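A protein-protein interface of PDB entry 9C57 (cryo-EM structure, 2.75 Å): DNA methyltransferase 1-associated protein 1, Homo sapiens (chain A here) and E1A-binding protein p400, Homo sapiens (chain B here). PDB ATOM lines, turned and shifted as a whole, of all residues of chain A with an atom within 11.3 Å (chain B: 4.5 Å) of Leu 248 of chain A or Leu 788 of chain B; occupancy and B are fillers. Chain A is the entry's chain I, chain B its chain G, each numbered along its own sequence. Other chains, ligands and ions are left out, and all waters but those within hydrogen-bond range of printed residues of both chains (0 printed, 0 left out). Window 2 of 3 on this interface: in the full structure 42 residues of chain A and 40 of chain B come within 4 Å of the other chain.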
ATOM      1  N   GLN A 229      -1.491  36.403   7.420  1.00  0.00           N
ATOM      2  CA  GLN A 229      -0.897  35.191   6.867  1.00  0.00           C
ATOM      3  C   GLN A 229      -0.529  34.209   7.971  1.00  0.00           C
ATOM      4  O   GLN A 229      -0.809  33.009   7.872  1.00  0.00           O
ATOM      5  CB  GLN A 229       0.330  35.556   6.030  1.00  0.00           C
ATOM      6  CG  GLN A 229       0.767  34.485   5.044  1.00  0.00           C
ATOM      7  CD  GLN A 229       1.919  33.653   5.565  1.00  0.00           C
ATOM      8  OE1 GLN A 229       2.116  33.534   6.773  1.00  0.00           O
ATOM      9  NE2 GLN A 229       2.695  33.079   4.652  1.00  0.00           N
ATOM     10  N   ARG A 232      -3.752  32.737   9.437  1.00  0.00           N
ATOM     11  CA  ARG A 232      -4.304  31.696   8.578  1.00  0.00           C
ATOM     12  C   ARG A 232      -3.476  30.422   8.664  1.00  0.00           C
ATOM     13  O   ARG A 232      -4.028  29.321   8.765  1.00  0.00           O
ATOM     14  CB  ARG A 232      -4.378  32.198   7.134  1.00  0.00           C
ATOM     15  CG  ARG A 232      -4.377  31.099   6.069  1.00  0.00           C
ATOM     16  CD  ARG A 232      -2.976  30.835   5.527  1.00  0.00           C
ATOM     17  NE  ARG A 232      -3.006  30.087   4.275  1.00  0.00           N
ATOM     18  CZ  ARG A 232      -2.731  28.794   4.158  1.00  0.00           C
ATOM     19  NH1 ARG A 232      -2.430  28.047   5.209  1.00  0.00           N
ATOM     20  NH2 ARG A 232      -2.762  28.233   2.953  1.00  0.00           N
ATOM     21  N   LEU A 233      -2.148  30.549   8.626  1.00  0.00           N
ATOM     22  CA  LEU A 233      -1.305  29.361   8.621  1.00  0.00           C
ATOM     23  C   LEU A 233      -1.462  28.571   9.912  1.00  0.00           C
ATOM     24  O   LEU A 233      -1.535  27.337   9.887  1.00  0.00           O
ATOM     25  CB  LEU A 233       0.157  29.751   8.405  1.00  0.00           C
ATOM     26  CG  LEU A 233       0.614  29.848   6.946  1.00  0.00           C
ATOM     27  CD1 LEU A 233       1.950  30.566   6.852  1.00  0.00           C
ATOM     28  CD2 LEU A 233       0.712  28.471   6.305  1.00  0.00           C
ATOM     29  N   TYR A 234      -1.521  29.260  11.052  1.00  0.00           N
ATOM     30  CA  TYR A 234      -1.585  28.560  12.330  1.00  0.00           C
ATOM     31  C   TYR A 234      -2.996  28.099  12.675  1.00  0.00           C
ATOM     32  O   TYR A 234      -3.170  26.991  13.195  1.00  0.00           O
ATOM     33  CB  TYR A 234      -1.035  29.446  13.449  1.00  0.00           C
ATOM     34  CG  TYR A 234      -0.316  28.663  14.528  1.00  0.00           C
ATOM     35  CD1 TYR A 234       0.865  27.985  14.249  1.00  0.00           C
ATOM     36  CD2 TYR A 234      -0.820  28.594  15.819  1.00  0.00           C
ATOM     37  CE1 TYR A 234       1.522  27.265  15.226  1.00  0.00           C
ATOM     38  CE2 TYR A 234      -0.166  27.877  16.803  1.00  0.00           C
ATOM     39  CZ  TYR A 234       1.003  27.214  16.500  1.00  0.00           C
ATOM     40  OH  TYR A 234       1.658  26.497  17.473  1.00  0.00           O
ATOM     41  N   ARG A 236      -5.002  27.037  10.734  1.00  0.00           N
ATOM     42  CA  ARG A 236      -5.206  25.882   9.871  1.00  0.00           C
ATOM     43  C   ARG A 236      -5.458  24.622  10.691  1.00  0.00           C
ATOM     44  O   ARG A 236      -4.689  24.293  11.598  1.00  0.00           O
ATOM     45  CB  ARG A 236      -3.966  25.711   8.997  1.00  0.00           C
ATOM     46  CG  ARG A 236      -4.019  24.590   7.992  1.00  0.00           C
ATOM     47  CD  ARG A 236      -2.860  24.698   6.995  1.00  0.00           C
ATOM     48  NE  ARG A 236      -1.627  25.195   7.600  1.00  0.00           N
ATOM     49  CZ  ARG A 236      -0.451  25.228   6.988  1.00  0.00           C
ATOM     50  NH1 ARG A 236      -0.305  24.798   5.746  1.00  0.00           N
ATOM     51  NH2 ARG A 236       0.605  25.707   7.639  1.00  0.00           N
ATOM     52  N   GLU A 239      -5.299  18.467  10.362  1.00  0.00           N
ATOM     53  CA  GLU A 239      -5.187  17.594   9.201  1.00  0.00           C
ATOM     54  C   GLU A 239      -4.755  18.383   7.973  1.00  0.00           C
ATOM     55  O   GLU A 239      -3.901  17.929   7.202  1.00  0.00           O
ATOM     56  CB  GLU A 239      -6.512  16.865   8.951  1.00  0.00           C
ATOM     57  CG  GLU A 239      -7.750  17.758   8.854  1.00  0.00           C
ATOM     58  CD  GLU A 239      -8.415  18.017  10.197  1.00  0.00           C
ATOM     59  OE1 GLU A 239      -7.991  17.417  11.207  1.00  0.00           O
ATOM     60  OE2 GLU A 239      -9.368  18.821  10.240  1.00  0.00           O
ATOM     61  N   GLN A 240      -5.317  19.579   7.787  1.00  0.00           N
ATOM     62  CA  GLN A 240      -4.937  20.377   6.630  1.00  0.00           C
ATOM     63  C   GLN A 240      -3.491  20.833   6.799  1.00  0.00           C
ATOM     64  O   GLN A 240      -2.734  20.900   5.831  1.00  0.00           O
ATOM     65  CB  GLN A 240      -5.873  21.583   6.500  1.00  0.00           C
ATOM     66  CG  GLN A 240      -5.474  22.701   5.515  1.00  0.00           C
ATOM     67  CD  GLN A 240      -4.891  22.202   4.191  1.00  0.00           C
ATOM     68  OE1 GLN A 240      -4.019  21.354   4.145  1.00  0.00           O
ATOM     69  NE2 GLN A 240      -5.387  22.766   3.096  1.00  0.00           N
ATOM     70  N   VAL A 241      -3.070  21.112   8.034  1.00  0.00           N
ATOM     71  CA  VAL A 241      -1.661  21.434   8.257  1.00  0.00           C
ATOM     72  C   VAL A 241      -0.788  20.320   7.703  1.00  0.00           C
ATOM     73  O   VAL A 241       0.116  20.555   6.894  1.00  0.00           O
ATOM     74  CB  VAL A 241      -1.367  21.677   9.751  1.00  0.00           C
ATOM     75  CG1 VAL A 241      -0.106  22.490   9.905  1.00  0.00           C
ATOM     76  CG2 VAL A 241      -2.489  22.429  10.432  1.00  0.00           C
ATOM     77  N   ALA A 242      -1.076  19.079   8.097  1.00  0.00           N
ATOM     78  CA  ALA A 242      -0.247  17.967   7.646  1.00  0.00           C
ATOM     79  C   ALA A 242      -0.289  17.830   6.127  1.00  0.00           C
ATOM     80  O   ALA A 242       0.754  17.703   5.472  1.00  0.00           O
ATOM     81  CB  ALA A 242      -0.695  16.671   8.322  1.00  0.00           C
ATOM     82  N   GLU A 243      -1.489  17.873   5.544  1.00  0.00           N
ATOM     83  CA  GLU A 243      -1.604  17.655   4.105  1.00  0.00           C
ATOM     84  C   GLU A 243      -0.904  18.757   3.318  1.00  0.00           C
ATOM     85  O   GLU A 243      -0.138  18.477   2.392  1.00  0.00           O
ATOM     86  CB  GLU A 243      -3.073  17.545   3.685  1.00  0.00           C
ATOM     87  CG  GLU A 243      -3.924  16.588   4.515  1.00  0.00           C
ATOM     88  CD  GLU A 243      -3.115  15.489   5.179  1.00  0.00           C
ATOM     89  OE1 GLU A 243      -2.874  15.581   6.400  1.00  0.00           O
ATOM     90  OE2 GLU A 243      -2.720  14.532   4.479  1.00  0.00           O
ATOM     91  N   GLU A 244      -1.158  20.022   3.664  1.00  0.00           N
ATOM     92  CA  GLU A 244      -0.536  21.125   2.940  1.00  0.00           C
ATOM     93  C   GLU A 244       0.977  21.106   3.097  1.00  0.00           C
ATOM     94  O   GLU A 244       1.707  21.288   2.116  1.00  0.00           O
ATOM     95  CB  GLU A 244      -1.105  22.461   3.416  1.00  0.00           C
ATOM     96  CG  GLU A 244      -0.929  23.593   2.414  1.00  0.00           C
ATOM     97  CD  GLU A 244      -1.554  24.893   2.883  1.00  0.00           C
ATOM     98  OE1 GLU A 244      -2.771  25.076   2.673  1.00  0.00           O
ATOM     99  OE2 GLU A 244      -0.830  25.730   3.461  1.00  0.00           O
ATOM    100  N   GLU A 245       1.474  20.882   4.317  1.00  0.00           N
ATOM    101  CA  GLU A 245       2.914  20.774   4.505  1.00  0.00           C
ATOM    102  C   GLU A 245       3.517  19.617   3.720  1.00  0.00           C
ATOM    103  O   GLU A 245       4.672  19.716   3.295  1.00  0.00           O
ATOM    104  CB  GLU A 245       3.235  20.663   5.996  1.00  0.00           C
ATOM    105  CG  GLU A 245       3.293  22.026   6.689  1.00  0.00           C
ATOM    106  CD  GLU A 245       1.936  22.689   6.824  1.00  0.00           C
ATOM    107  OE1 GLU A 245       1.116  22.565   5.890  1.00  0.00           O
ATOM    108  OE2 GLU A 245       1.696  23.350   7.855  1.00  0.00           O
ATOM    109  N   TYR A 246       2.777  18.527   3.507  1.00  0.00           N
ATOM    110  CA  TYR A 246       3.232  17.532   2.541  1.00  0.00           C
ATOM    111  C   TYR A 246       3.272  18.150   1.145  1.00  0.00           C
ATOM    112  O   TYR A 246       4.293  18.095   0.451  1.00  0.00           O
ATOM    113  CB  TYR A 246       2.316  16.302   2.566  1.00  0.00           C
ATOM    114  CG  TYR A 246       2.473  15.339   1.390  1.00  0.00           C
ATOM    115  CD1 TYR A 246       3.644  15.293   0.634  1.00  0.00           C
ATOM    116  CD2 TYR A 246       1.474  14.425   1.086  1.00  0.00           C
ATOM    117  CE1 TYR A 246       3.786  14.411  -0.421  1.00  0.00           C
ATOM    118  CE2 TYR A 246       1.608  13.538   0.032  1.00  0.00           C
ATOM    119  CZ  TYR A 246       2.767  13.532  -0.714  1.00  0.00           C
ATOM    120  OH  TYR A 246       2.907  12.646  -1.759  1.00  0.00           O
ATOM    121  N   LEU A 247       2.159  18.756   0.726  1.00  0.00           N
ATOM    122  CA  LEU A 247       2.115  19.440  -0.558  1.00  0.00           C
ATOM    123  C   LEU A 247       3.182  20.519  -0.637  1.00  0.00           C
ATOM    124  O   LEU A 247       3.676  20.832  -1.725  1.00  0.00           O
ATOM    125  CB  LEU A 247       0.731  20.060  -0.773  1.00  0.00           C
ATOM    126  CG  LEU A 247      -0.461  19.100  -0.800  1.00  0.00           C
ATOM    127  CD1 LEU A 247      -1.775  19.869  -0.759  1.00  0.00           C
ATOM    128  CD2 LEU A 247      -0.407  18.208  -2.026  1.00  0.00           C
ATOM    129  N   LEU A 248       3.548  21.094   0.508  1.00  0.00           N
ATOM    130  CA  LEU A 248       4.540  22.162   0.527  1.00  0.00           C
ATOM    131  C   LEU A 248       5.888  21.668   0.018  1.00  0.00           C
ATOM    132  O   LEU A 248       6.524  22.311  -0.824  1.00  0.00           O
ATOM    133  CB  LEU A 248       4.670  22.705   1.951  1.00  0.00           C
ATOM    134  CG  LEU A 248       4.794  24.206   2.210  1.00  0.00           C
ATOM    135  CD1 LEU A 248       3.956  24.990   1.234  1.00  0.00           C
ATOM    136  CD2 LEU A 248       4.385  24.524   3.640  1.00  0.00           C
ATOM    137  N   GLN A 249       6.337  20.516   0.519  1.00  0.00           N
ATOM    138  CA  GLN A 249       7.676  20.027   0.217  1.00  0.00           C
ATOM    139  C   GLN A 249       7.744  19.218  -1.070  1.00  0.00           C
ATOM    140  O   GLN A 249       8.807  19.173  -1.698  1.00  0.00           O
ATOM    141  CB  GLN A 249       8.192  19.172   1.377  1.00  0.00           C
ATOM    142  CG  GLN A 249       7.387  17.898   1.624  1.00  0.00           C
ATOM    143  CD  GLN A 249       7.826  16.736   0.750  1.00  0.00           C
ATOM    144  OE1 GLN A 249       8.819  16.825   0.028  1.00  0.00           O
ATOM    145  NE2 GLN A 249       7.078  15.640   0.806  1.00  0.00           N
ATOM    146  N   GLU A 250       6.647  18.576  -1.475  1.00  0.00           N
ATOM    147  CA  GLU A 250       6.720  17.619  -2.572  1.00  0.00           C
ATOM    148  C   GLU A 250       7.227  18.276  -3.851  1.00  0.00           C
ATOM    149  O   GLU A 250       8.128  17.750  -4.514  1.00  0.00           O
ATOM    150  CB  GLU A 250       5.349  16.980  -2.801  1.00  0.00           C
ATOM    151  CG  GLU A 250       5.374  15.786  -3.743  1.00  0.00           C
ATOM    152  CD  GLU A 250       6.349  14.711  -3.301  1.00  0.00           C
ATOM    153  OE1 GLU A 250       6.534  14.542  -2.077  1.00  0.00           O
ATOM    154  OE2 GLU A 250       6.935  14.042  -4.177  1.00  0.00           O
ATOM    155  N   LEU A 251       6.665  19.425  -4.211  1.00  0.00           N
ATOM    156  CA  LEU A 251       7.100  20.129  -5.413  1.00  0.00           C
ATOM    157  C   LEU A 251       8.327  20.981  -5.109  1.00  0.00           C
ATOM    158  O   LEU A 251       9.242  21.082  -5.925  1.00  0.00           O
ATOM    159  CB  LEU A 251       5.978  21.007  -5.983  1.00  0.00           C
ATOM    160  CG  LEU A 251       5.610  22.308  -5.258  1.00  0.00           C
ATOM    161  CD1 LEU A 251       4.484  23.011  -6.000  1.00  0.00           C
ATOM    162  CD2 LEU A 251       5.215  22.066  -3.817  1.00  0.00           C
ATOM    163  N   ARG B 784      -0.855  19.515  -6.757  1.00  0.00           N
ATOM    164  CA  ARG B 784      -0.100  20.233  -5.739  1.00  0.00           C
ATOM    165  C   ARG B 784       0.412  21.557  -6.287  1.00  0.00           C
ATOM    166  O   ARG B 784       0.376  22.581  -5.596  1.00  0.00           O
ATOM    167  CB  ARG B 784       1.075  19.385  -5.242  1.00  0.00           C
ATOM    168  CG  ARG B 784       0.833  17.880  -5.204  1.00  0.00           C
ATOM    169  CD  ARG B 784       1.983  17.157  -4.518  1.00  0.00           C
ATOM    170  NE  ARG B 784       1.692  15.746  -4.292  1.00  0.00           N
ATOM    171  CZ  ARG B 784       1.825  14.796  -5.208  1.00  0.00           C
ATOM    172  NH1 ARG B 784       2.233  15.071  -6.437  1.00  0.00           N
ATOM    173  NH2 ARG B 784       1.542  13.537  -4.885  1.00  0.00           N
ATOM    174  N   ILE B 785       0.893  21.554  -7.532  1.00  0.00           N
ATOM    175  CA  ILE B 785       1.451  22.769  -8.119  1.00  0.00           C
ATOM    176  C   ILE B 785       0.389  23.859  -8.189  1.00  0.00           C
ATOM    177  O   ILE B 785       0.623  25.002  -7.783  1.00  0.00           O
ATOM    178  CB  ILE B 785       2.044  22.468  -9.506  1.00  0.00           C
ATOM    179  CG1 ILE B 785       3.172  21.437  -9.385  1.00  0.00           C
ATOM    180  CG2 ILE B 785       2.554  23.751 -10.155  1.00  0.00           C
ATOM    181  CD1 ILE B 785       3.719  20.957 -10.714  1.00  0.00           C
ATOM    182  N   ALA B 786      -0.795  23.523  -8.707  1.00  0.00           N
ATOM    183  CA  ALA B 786      -1.864  24.512  -8.808  1.00  0.00           C
ATOM    184  C   ALA B 786      -2.331  24.957  -7.428  1.00  0.00           C
ATOM    185  O   ALA B 786      -2.539  26.153  -7.181  1.00  0.00           O
ATOM    186  CB  ALA B 786      -3.031  23.936  -9.611  1.00  0.00           C
ATOM    187  N   GLU B 787      -2.503  24.001  -6.511  1.00  0.00           N
ATOM    188  CA  GLU B 787      -2.966  24.336  -5.170  1.00  0.00           C
ATOM    189  C   GLU B 787      -2.007  25.300  -4.488  1.00  0.00           C
ATOM    190  O   GLU B 787      -2.434  26.228  -3.791  1.00  0.00           O
ATOM    191  CB  GLU B 787      -3.126  23.059  -4.343  1.00  0.00           C
ATOM    192  CG  GLU B 787      -3.744  23.272  -2.973  1.00  0.00           C
ATOM    193  CD  GLU B 787      -5.179  23.746  -3.050  1.00  0.00           C
ATOM    194  OE1 GLU B 787      -5.786  23.629  -4.135  1.00  0.00           O
ATOM    195  OE2 GLU B 787      -5.702  24.235  -2.027  1.00  0.00           O
ATOM    196  N   LEU B 788      -0.704  25.090  -4.669  1.00  0.00           N
ATOM    197  CA  LEU B 788       0.285  25.985  -4.088  1.00  0.00           C
ATOM    198  C   LEU B 788       0.343  27.319  -4.818  1.00  0.00           C
ATOM    199  O   LEU B 788       0.542  28.361  -4.183  1.00  0.00           O
ATOM    200  CB  LEU B 788       1.660  25.318  -4.106  1.00  0.00           C
ATOM    201  CG  LEU B 788       2.017  24.542  -2.838  1.00  0.00           C
ATOM    202  CD1 LEU B 788       2.199  25.499  -1.680  1.00  0.00           C
ATOM    203  CD2 LEU B 788       0.961  23.496  -2.508  1.00  0.00           C
ATOM    204  N   ARG B 789       0.177  27.310  -6.142  1.00  0.00           N
ATOM    205  CA  ARG B 789       0.218  28.553  -6.901  1.00  0.00           C
ATOM    206  C   ARG B 789      -0.905  29.485  -6.473  1.00  0.00           C
ATOM    207  O   ARG B 789      -0.671  30.660  -6.169  1.00  0.00           O
ATOM    208  CB  ARG B 789       0.129  28.249  -8.396  1.00  0.00           C
ATOM    209  CG  ARG B 789       1.417  27.708  -8.996  1.00  0.00           C
ATOM    210  CD  ARG B 789       2.415  28.819  -9.278  1.00  0.00           C
ATOM    211  NE  ARG B 789       1.963  29.702 -10.348  1.00  0.00           N
ATOM    212  CZ  ARG B 789       2.660  30.727 -10.820  1.00  0.00           C
ATOM    213  NH1 ARG B 789       3.855  31.031 -10.342  1.00  0.00           N
ATOM    214  NH2 ARG B 789       2.143  31.466 -11.798  1.00  0.00           N
ATOM    215  N   LYS B 790      -2.139  28.977  -6.437  1.00  0.00           N
ATOM    216  CA  LYS B 790      -3.246  29.818  -5.993  1.00  0.00           C
ATOM    217  C   LYS B 790      -3.076  30.215  -4.533  1.00  0.00           C
ATOM    218  O   LYS B 790      -3.284  31.380  -4.171  1.00  0.00           O
ATOM    219  CB  LYS B 790      -4.580  29.101  -6.206  1.00  0.00           C
ATOM    220  CG  LYS B 790      -4.776  27.856  -5.357  1.00  0.00           C
ATOM    221  CD  LYS B 790      -5.589  28.157  -4.103  1.00  0.00           C
ATOM    222  CE  LYS B 790      -5.644  26.957  -3.177  1.00  0.00           C
ATOM    223  NZ  LYS B 790      -6.450  27.227  -1.956  1.00  0.00           N
ATOM    224  N   ALA B 791      -2.688  29.264  -3.679  1.00  0.00           N
ATOM    225  CA  ALA B 791      -2.478  29.576  -2.270  1.00  0.00           C
ATOM    226  C   ALA B 791      -1.275  30.491  -2.084  1.00  0.00           C
ATOM    227  O   ALA B 791      -1.303  31.399  -1.246  1.00  0.00           O
ATOM    228  CB  ALA B 791      -2.300  28.286  -1.471  1.00  0.00           C
ATOM    229  N   GLY B 792      -0.214  30.271  -2.861  1.00  0.00           N
ATOM    230  CA  GLY B 792       0.984  31.084  -2.751  1.00  0.00           C
ATOM    231  C   GLY B 792       0.789  32.533  -3.143  1.00  0.00           C
ATOM    232  O   GLY B 792       1.667  33.356  -2.864  1.00  0.00           O
ATOM    233  N   GLN B 796       0.814  31.460   1.207  1.00  0.00           N
ATOM    234  CA  GLN B 796       1.805  30.407   1.395  1.00  0.00           C
ATOM    235  C   GLN B 796       3.159  30.846   0.859  1.00  0.00           C
ATOM    236  O   GLN B 796       3.269  31.794   0.078  1.00  0.00           O
ATOM    237  CB  GLN B 796       1.370  29.110   0.707  1.00  0.00           C
ATOM    238  CG  GLN B 796       0.836  28.049   1.652  1.00  0.00           C
ATOM    239  CD  GLN B 796       1.909  27.494   2.566  1.00  0.00           C
ATOM    240  OE1 GLN B 796       3.026  28.006   2.613  1.00  0.00           O
ATOM    241  NE2 GLN B 796       1.575  26.434   3.292  1.00  0.00           N
ATOM    242  N   ARG B 797       4.190  30.129   1.303  1.00  0.00           N
ATOM    243  CA  ARG B 797       5.555  30.110   0.795  1.00  0.00           C
ATOM    244  C   ARG B 797       6.370  31.334   1.190  1.00  0.00           C
ATOM    245  O   ARG B 797       7.562  31.372   0.886  1.00  0.00           O
ATOM    246  CB  ARG B 797       5.624  29.955  -0.737  1.00  0.00           C
ATOM    247  CG  ARG B 797       4.777  28.820  -1.287  1.00  0.00           C
ATOM    248  CD  ARG B 797       4.810  27.566  -0.415  1.00  0.00           C
ATOM    249  NE  ARG B 797       6.161  27.153  -0.039  1.00  0.00           N
ATOM    250  CZ  ARG B 797       6.591  26.959   1.204  1.00  0.00           C
ATOM    251  NH1 ARG B 797       5.809  27.160   2.254  1.00  0.00           N
ATOM    252  NH2 ARG B 797       7.844  26.559   1.400  1.00  0.00           N
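NE2 of Gln 796 of chain B lies within hydrogen-bond range of OE2 of Glu 244 of chain A (2.5 Å). The guanidinium group (NH1) of Arg 236 of chain A sits close to the side-chain amide nitrogen (NE2) of Gln 796 of chain B, at 3.5 Å.
Among the printed residues, merely in contact across the chains: Leu 248 of chain A with Arg 797 of chain B (3.0 Å), Leu 248 of chain A with Gln 796 of chain B (3.4 Å), Leu 247 of chain A with Arg 784 of chain B (3.4 Å), Leu 248 of chain A with Leu 788 of chain B (3.4 Å), Tyr 246 of chain A with Arg 784 of chain B (3.5 Å), Leu 251 of chain A with Ile 785 of chain B (3.7 Å), Glu 250 of chain A with Arg 784 of chain B (3.7 Å), Leu 233 of chain A with Gln 796 of chain B (3.7 Å), Arg 232 of chain A with Gln 796 of chain B (3.8 Å) and Leu 247 of chain A with Leu 788 of chain B (3.9 Å).
Of the 11 printed residues of chain B, 5 touch a printed residue of chain A. Printed residues of chain B that touch a printed residue of chain A: Arg 784, Ile 785, Leu 788, Gln 796 and Arg 797. Hydrophobic or aromatic side chains of chain B within 4 Å of the printed part of chain A: Ile 785 and Leu 788. Along chain B the printed residues that touch a printed residue of chain A span positions 784 to 797. Of the 18 printed residues of chain A, 9 touch a printed residue of chain B. Hydrophobic or aromatic side chains of chain A within 4 Å of the printed part of chain B: Leu 233, Tyr 246, Leu 247, Leu 248 and Leu 251.
The side-chain carboxylate of Glu 245 of chain A is in salt-bridge range of the guanidinium group of Arg 236 of chain A (2.6 Å). The guanidinium group (NH2) of Arg 232 of chain A is in salt-bridge range of the side-chain carboxylate (OE1) of Glu 244 of chain A (3.2 Å). O of Ala 791 of chain B lies within hydrogen-bond range of N of Gln 796 of chain B (3.2 Å). The guanidinium group of Arg 236 of chain A sits close to the backbone carbonyl oxygen of Leu 233 of chain A, 3.1 Å away. The guanidinium group of Arg 236 of chain A lies within salt-bridge range of the side-chain carboxylate of Glu 244 of chain A (2.5 Å). The side-chain amide nitrogen of Gln 249 of chain A sits at hydrogen-bond distance from the side-chain carboxylate of Glu 250 of chain A, 3.1 Å away.
Of the printed residues of chain B, Leu 248 of chain A touches Leu 788, Gln 796 and Arg 797. Of the printed residues of chain A, Leu 788 of chain B touches Leu 247 and Leu 248. No residue of chain A comes within 4 Å of Glu 787 of chain B. No residue of chain A comes within 4 Å of Lys 790 of chain B. No residue of chain A comes within 4 Å of Ala 791 of chain B. Gln 796 of chain B touches just these residues of chain A: Arg 232, Leu 233, Arg 236, Glu 244 and Leu 248. Of the printed residues of chain B, Arg 232 of chain A touches Gln 796. Printed residues of chain B within 4 Å of Arg 236 of chain A: Gln 796 (3.5 Å). Of the printed residues of chain B, Glu 244 of chain A touches Gln 796. The nearest printed residue of chain B that does not touch Leu 248 of chain A is Arg 784 of chain B (6.5 Å). The nearest residue of chain A that does not touch Leu 788 of chain B is Leu 251 of chain A (4.1 Å).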
